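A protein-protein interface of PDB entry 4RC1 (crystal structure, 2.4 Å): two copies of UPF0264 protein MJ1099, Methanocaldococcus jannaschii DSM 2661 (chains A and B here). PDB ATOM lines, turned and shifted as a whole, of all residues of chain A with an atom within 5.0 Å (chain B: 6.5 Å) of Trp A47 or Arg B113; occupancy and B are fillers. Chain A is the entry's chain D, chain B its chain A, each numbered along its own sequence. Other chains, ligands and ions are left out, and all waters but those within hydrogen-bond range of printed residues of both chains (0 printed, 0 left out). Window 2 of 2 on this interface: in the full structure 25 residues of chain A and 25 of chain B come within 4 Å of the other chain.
The guanidinium group (NE) of Arg B113 lies within salt-bridge range of the side-chain carboxylate (OD2) of Asp B117 (3.7 Å).
O of Asn B110 lies close to OG of Ser B77.
The indole nitrogen of Trp A47 sits close to the guanidinium group of Arg B113, 3.2 Å away.
Among the printed residues, merely in contact across the chains: Phe A45 with Ser B77, Phe A45 with Asn B110, Pro A46 with Ser B77, Pro A46 with Leu B78, Pro A46 with Ala B114, Trp A47 with Asn B110, Trp A47 with Ala B114 and Ile A49 with Leu B78.
No position is printed for both chains.
Of the 9 pairs that touch across the chains among the printed residues, none has its exchanged pair printed and touching as well.
Trp A47 touches three residues of chain B.
Of chain A, only Trp A47 (3.2 Å) comes within 4 Å of Arg B113.
Of the printed residues of chain A, Ala B114 touches Pro A46 (3.8 Å) and Trp A47 (3.7 Å).
Of the printed residues of chain B, Phe A45 touches Ser B77 and Asn B110.
Lys B116 touches none of the printed residues of chain A.
The nearest residue of chain B that does not touch Trp A47 is Asp B117 (4.1 Å).
The nearest printed residue of chain B that does not touch Ile A49 is Ser B77 (8.4 Å).
Hydrophobic or aromatic side chains of chain A that line the printed part of chain B: Phe A45, Pro A46, Trp A47 and Ile A49.
Printed residues of chain B that touch a printed residue of chain A: Ser B77, Leu B78, Asn B110, Arg B113 and Ala B114.
Hydrophobic or aromatic side chains of chain B within 4 Å of the printed part of chain A: Leu B78 and Ala B114.
Among the printed residues, no Asp or Glu carboxylate lies within 4 Å of a Lys or Arg side-chain nitrogen of the other chain.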
ATOM      1  N   PHE A  45      -5.428  11.619  15.572  1.00  0.00           N
ATOM      2  CA  PHE A  45      -5.375  12.375  16.813  1.00  0.00           C
ATOM      3  C   PHE A  45      -5.288  13.879  16.659  1.00  0.00           C
ATOM      4  O   PHE A  45      -4.726  14.335  15.672  1.00  0.00           O
ATOM      5  CB  PHE A  45      -4.263  11.819  17.690  1.00  0.00           C
ATOM      6  CG  PHE A  45      -4.536  10.371  18.041  1.00  0.00           C
ATOM      7  CD1 PHE A  45      -5.507  10.037  18.984  1.00  0.00           C
ATOM      8  CD2 PHE A  45      -3.853   9.343  17.400  1.00  0.00           C
ATOM      9  CE1 PHE A  45      -5.799   8.702  19.265  1.00  0.00           C
ATOM     10  CE2 PHE A  45      -4.148   8.002  17.682  1.00  0.00           C
ATOM     11  CZ  PHE A  45      -5.114   7.691  18.622  1.00  0.00           C
ATOM     12  N   PRO A  46      -5.824  14.678  17.622  1.00  0.00           N
ATOM     13  CA  PRO A  46      -5.726  16.157  17.497  1.00  0.00           C
ATOM     14  C   PRO A  46      -4.312  16.693  17.244  1.00  0.00           C
ATOM     15  O   PRO A  46      -4.150  17.626  16.443  1.00  0.00           O
ATOM     16  CB  PRO A  46      -6.311  16.673  18.823  1.00  0.00           C
ATOM     17  CG  PRO A  46      -6.369  15.475  19.729  1.00  0.00           C
ATOM     18  CD  PRO A  46      -6.550  14.295  18.852  1.00  0.00           C
ATOM     19  N   TRP A  47      -3.290  16.084  17.887  1.00  0.00           N
ATOM     20  CA  TRP A  47      -1.887  16.508  17.724  1.00  0.00           C
ATOM     21  C   TRP A  47      -1.347  16.220  16.324  1.00  0.00           C
ATOM     22  O   TRP A  47      -0.531  16.989  15.827  1.00  0.00           O
ATOM     23  CB  TRP A  47      -0.972  15.915  18.813  1.00  0.00           C
ATOM     24  CG  TRP A  47      -1.127  14.429  19.025  1.00  0.00           C
ATOM     25  CD1 TRP A  47      -0.406  13.432  18.430  1.00  0.00           C
ATOM     26  CD2 TRP A  47      -2.033  13.784  19.930  1.00  0.00           C
ATOM     27  NE1 TRP A  47      -0.815  12.203  18.895  1.00  0.00           N
ATOM     28  CE2 TRP A  47      -1.805  12.386  19.828  1.00  0.00           C
ATOM     29  CE3 TRP A  47      -3.021  14.249  20.818  1.00  0.00           C
ATOM     30  CZ2 TRP A  47      -2.525  11.447  20.590  1.00  0.00           C
ATOM     31  CZ3 TRP A  47      -3.759  13.316  21.542  1.00  0.00           C
ATOM     32  CH2 TRP A  47      -3.506  11.934  21.429  1.00  0.00           C
ATOM     33  N   MET A  48      -1.819  15.139  15.677  1.00  0.00           N
ATOM     34  CA  MET A  48      -1.405  14.762  14.322  1.00  0.00           C
ATOM     35  C   MET A  48      -1.969  15.728  13.287  1.00  0.00           C
ATOM     36  O   MET A  48      -1.250  16.105  12.374  1.00  0.00           O
ATOM     37  CB  MET A  48      -1.800  13.299  14.014  1.00  0.00           C
ATOM     38  CG  MET A  48      -1.210  12.759  12.727  1.00  0.00           C
ATOM     39  SD  MET A  48       0.601  12.824  12.683  1.00  0.00           S
ATOM     40  CE  MET A  48       0.999  11.443  13.739  1.00  0.00           C
ATOM     41  N   ILE A  49      -3.245  16.139  13.443  1.00  0.00           N
ATOM     42  CA  ILE A  49      -3.938  17.094  12.565  1.00  0.00           C
ATOM     43  C   ILE A  49      -3.198  18.427  12.643  1.00  0.00           C
ATOM     44  O   ILE A  49      -2.916  19.015  11.599  1.00  0.00           O
ATOM     45  CB  ILE A  49      -5.465  17.211  12.898  1.00  0.00           C
ATOM     46  CG1 ILE A  49      -6.188  15.833  12.737  1.00  0.00           C
ATOM     47  CG2 ILE A  49      -6.146  18.302  12.057  1.00  0.00           C
ATOM     48  CD1 ILE A  49      -7.599  15.730  13.364  1.00  0.00           C
ATOM     49  N   LYS A  50      -2.815  18.859  13.878  1.00  0.00           N
ATOM     50  CA  LYS A  50      -2.072  20.095  14.130  1.00  0.00           C
ATOM     51  C   LYS A  50      -0.679  20.049  13.506  1.00  0.00           C
ATOM     52  O   LYS A  50      -0.289  21.010  12.844  1.00  0.00           O
ATOM     53  CB  LYS A  50      -2.008  20.389  15.635  1.00  0.00           C
ATOM     54  CG  LYS A  50      -1.526  21.792  15.978  1.00  0.00           C
ATOM     55  CD  LYS A  50      -1.387  21.997  17.484  1.00  0.00           C
ATOM     56  CE  LYS A  50      -0.490  23.173  17.844  1.00  0.00           C
ATOM     57  NZ  LYS A  50       0.446  22.882  18.976  1.00  0.00           N
ATOM     58  N   ALA A  51       0.062  18.939  13.705  1.00  0.00           N
ATOM     59  CA  ALA A  51       1.415  18.745  13.164  1.00  0.00           C
ATOM     60  C   ALA A  51       1.419  18.764  11.631  1.00  0.00           C
ATOM     61  O   ALA A  51       2.314  19.368  11.032  1.00  0.00           O
ATOM     62  CB  ALA A  51       2.015  17.448  13.680  1.00  0.00           C
ATOM     63  N   SER B  77     -10.663  11.211  21.359  1.00  0.00           N
ATOM     64  CA  SER B  77      -9.648  12.234  21.677  1.00  0.00           C
ATOM     65  C   SER B  77     -10.110  13.583  21.091  1.00  0.00           C
ATOM     66  O   SER B  77     -10.017  14.605  21.764  1.00  0.00           O
ATOM     67  CB  SER B  77      -8.291  11.871  21.083  1.00  0.00           C
ATOM     68  OG  SER B  77      -7.798  10.703  21.702  1.00  0.00           O
ATOM     69  N   LEU B  78     -10.633  13.562  19.855  1.00  0.00           N
ATOM     70  CA  LEU B  78     -11.161  14.747  19.188  1.00  0.00           C
ATOM     71  C   LEU B  78     -12.396  15.269  19.930  1.00  0.00           C
ATOM     72  O   LEU B  78     -12.507  16.466  20.144  1.00  0.00           O
ATOM     73  CB  LEU B  78     -11.476  14.454  17.717  1.00  0.00           C
ATOM     74  CG  LEU B  78     -10.279  14.199  16.759  1.00  0.00           C
ATOM     75  CD1 LEU B  78     -10.777  13.716  15.408  1.00  0.00           C
ATOM     76  CD2 LEU B  78      -9.425  15.454  16.571  1.00  0.00           C
ATOM     77  N   MET B 108      -8.032   5.858  26.843  1.00  0.00           N
ATOM     78  CA  MET B 108      -7.882   6.840  27.923  1.00  0.00           C
ATOM     79  C   MET B 108      -6.575   7.652  27.896  1.00  0.00           C
ATOM     80  O   MET B 108      -6.627   8.861  28.158  1.00  0.00           O
ATOM     81  CB  MET B 108      -8.139   6.213  29.311  1.00  0.00           C
ATOM     82  CG  MET B 108      -9.580   5.787  29.558  1.00  0.00           C
ATOM     83  SD  MET B 108     -10.862   7.014  29.193  1.00  0.00           S
ATOM     84  CE  MET B 108     -10.398   8.362  30.252  1.00  0.00           C
ATOM     85  N   LYS B 109      -5.421   7.003  27.551  1.00  0.00           N
ATOM     86  CA  LYS B 109      -4.097   7.659  27.429  1.00  0.00           C
ATOM     87  C   LYS B 109      -4.177   8.771  26.376  1.00  0.00           C
ATOM     88  O   LYS B 109      -3.653   9.855  26.586  1.00  0.00           O
ATOM     89  CB  LYS B 109      -3.024   6.659  26.974  1.00  0.00           C
ATOM     90  CG  LYS B 109      -2.250   5.999  28.087  1.00  0.00           C
ATOM     91  CD  LYS B 109      -1.224   5.018  27.533  1.00  0.00           C
ATOM     92  CE  LYS B 109      -0.356   4.400  28.604  1.00  0.00           C
ATOM     93  NZ  LYS B 109       0.605   5.380  29.175  1.00  0.00           N
ATOM     94  N   ASN B 110      -4.885   8.503  25.257  1.00  0.00           N
ATOM     95  CA  ASN B 110      -5.072   9.460  24.172  1.00  0.00           C
ATOM     96  C   ASN B 110      -5.995  10.614  24.540  1.00  0.00           C
ATOM     97  O   ASN B 110      -5.715  11.756  24.167  1.00  0.00           O
ATOM     98  CB  ASN B 110      -5.483   8.754  22.891  1.00  0.00           C
ATOM     99  CG  ASN B 110      -4.353   7.929  22.310  1.00  0.00           C
ATOM    100  OD1 ASN B 110      -4.458   6.728  22.131  1.00  0.00           O
ATOM    101  ND2 ASN B 110      -3.256   8.552  21.980  1.00  0.00           N
ATOM    102  N   VAL B 111      -7.063  10.328  25.304  1.00  0.00           N
ATOM    103  CA  VAL B 111      -7.995  11.358  25.793  1.00  0.00           C
ATOM    104  C   VAL B 111      -7.238  12.304  26.793  1.00  0.00           C
ATOM    105  O   VAL B 111      -7.334  13.531  26.675  1.00  0.00           O
ATOM    106  CB  VAL B 111      -9.254  10.709  26.439  1.00  0.00           C
ATOM    107  CG1 VAL B 111     -10.076  11.735  27.229  1.00  0.00           C
ATOM    108  CG2 VAL B 111     -10.116   9.997  25.390  1.00  0.00           C
ATOM    109  N   VAL B 112      -6.442  11.705  27.713  1.00  0.00           N
ATOM    110  CA  VAL B 112      -5.641  12.417  28.704  1.00  0.00           C
ATOM    111  C   VAL B 112      -4.673  13.367  27.977  1.00  0.00           C
ATOM    112  O   VAL B 112      -4.632  14.543  28.310  1.00  0.00           O
ATOM    113  CB  VAL B 112      -4.944  11.433  29.712  1.00  0.00           C
ATOM    114  CG1 VAL B 112      -3.838  12.122  30.529  1.00  0.00           C
ATOM    115  CG2 VAL B 112      -5.968  10.764  30.641  1.00  0.00           C
ATOM    116  N   ARG B 113      -3.954  12.878  26.958  1.00  0.00           N
ATOM    117  CA  ARG B 113      -3.028  13.684  26.159  1.00  0.00           C
ATOM    118  C   ARG B 113      -3.747  14.843  25.466  1.00  0.00           C
ATOM    119  O   ARG B 113      -3.275  15.962  25.544  1.00  0.00           O
ATOM    120  CB  ARG B 113      -2.270  12.834  25.119  1.00  0.00           C
ATOM    121  CG  ARG B 113      -1.167  13.643  24.457  1.00  0.00           C
ATOM    122  CD  ARG B 113      -0.519  12.975  23.272  1.00  0.00           C
ATOM    123  NE  ARG B 113       0.318  13.948  22.573  1.00  0.00           N
ATOM    124  CZ  ARG B 113       1.192  13.643  21.629  1.00  0.00           C
ATOM    125  NH1 ARG B 113       1.369  12.381  21.265  1.00  0.00           N
ATOM    126  NH2 ARG B 113       1.902  14.597  21.045  1.00  0.00           N
ATOM    127  N   ALA B 114      -4.879  14.574  24.795  1.00  0.00           N
ATOM    128  CA  ALA B 114      -5.684  15.561  24.079  1.00  0.00           C
ATOM    129  C   ALA B 114      -6.152  16.688  25.011  1.00  0.00           C
ATOM    130  O   ALA B 114      -6.031  17.853  24.659  1.00  0.00           O
ATOM    131  CB  ALA B 114      -6.883  14.873  23.426  1.00  0.00           C
ATOM    132  N   VAL B 115      -6.658  16.335  26.189  1.00  0.00           N
ATOM    133  CA  VAL B 115      -7.166  17.265  27.218  1.00  0.00           C
ATOM    134  C   VAL B 115      -6.027  18.038  27.910  1.00  0.00           C
ATOM    135  O   VAL B 115      -6.094  19.269  27.972  1.00  0.00           O
ATOM    136  CB  VAL B 115      -8.115  16.552  28.225  1.00  0.00           C
ATOM    137  CG1 VAL B 115      -8.431  17.432  29.421  1.00  0.00           C
ATOM    138  CG2 VAL B 115      -9.402  16.109  27.538  1.00  0.00           C
ATOM    139  N   LYS B 116      -4.973  17.328  28.415  1.00  0.00           N
ATOM    140  CA  LYS B 116      -3.858  17.983  29.095  1.00  0.00           C
ATOM    141  C   LYS B 116      -3.065  18.901  28.167  1.00  0.00           C
ATOM    142  O   LYS B 116      -2.502  19.871  28.657  1.00  0.00           O
ATOM    143  CB  LYS B 116      -2.947  16.994  29.849  1.00  0.00           C
ATOM    144  CG  LYS B 116      -3.620  16.090  30.887  1.00  0.00           C
ATOM    145  CD  LYS B 116      -4.109  16.768  32.164  1.00  0.00           C
ATOM    146  CE  LYS B 116      -4.764  15.773  33.103  1.00  0.00           C
ATOM    147  NZ  LYS B 116      -5.144  16.415  34.398  1.00  0.00           N
ATOM    148  N   ASP B 117      -3.062  18.638  26.838  1.00  0.00           N
ATOM    149  CA  ASP B 117      -2.384  19.491  25.855  1.00  0.00           C
ATOM    150  C   ASP B 117      -3.088  20.845  25.749  1.00  0.00           C
ATOM    151  O   ASP B 117      -2.435  21.836  25.426  1.00  0.00           O
ATOM    152  CB  ASP B 117      -2.330  18.836  24.460  1.00  0.00           C
ATOM    153  CG  ASP B 117      -1.220  17.832  24.191  1.00  0.00           C
ATOM    154  OD1 ASP B 117      -0.384  17.615  25.090  1.00  0.00           O
ATOM    155  OD2 ASP B 117      -1.228  17.214  23.094  1.00  0.00           O
ATOM    156  N   ILE B 118      -4.412  20.889  26.016  1.00  0.00           N
ATOM    157  CA  ILE B 118      -5.202  22.123  26.007  1.00  0.00           C
ATOM    158  C   ILE B 118      -4.978  22.851  27.347  1.00  0.00           C
ATOM    159  O   ILE B 118      -4.614  24.026  27.345  1.00  0.00           O
ATOM    160  CB  ILE B 118      -6.697  21.833  25.714  1.00  0.00           C
ATOM    161  CG1 ILE B 118      -6.895  21.323  24.259  1.00  0.00           C
ATOM    162  CG2 ILE B 118      -7.570  23.074  25.983  1.00  0.00           C
ATOM    163  CD1 ILE B 118      -8.076  20.523  24.112  1.00  0.00           C
ATOM    164  N   VAL B 124      -9.659  14.485  33.844  1.00  0.00           N
ATOM    165  CA  VAL B 124     -10.059  13.358  33.016  1.00  0.00           C
ATOM    166  C   VAL B 124     -10.585  12.203  33.913  1.00  0.00           C
ATOM    167  O   VAL B 124      -9.912  11.737  34.853  1.00  0.00           O
ATOM    168  CB  VAL B 124      -8.985  12.909  32.007  1.00  0.00           C
ATOM    169  CG1 VAL B 124      -9.525  11.792  31.106  1.00  0.00           C
ATOM    170  CG2 VAL B 124      -8.499  14.101  31.169  1.00  0.00           C
ATOM    171  N   ALA B 150      -3.571   5.066  32.625  1.00  0.00           N
ATOM    172  CA  ALA B 150      -3.831   6.020  31.546  1.00  0.00           C
ATOM    173  C   ALA B 150      -3.543   7.459  31.987  1.00  0.00           C
ATOM    174  O   ALA B 150      -3.492   8.361  31.154  1.00  0.00           O
ATOM    175  CB  ALA B 150      -5.265   5.880  31.048  1.00  0.00           C
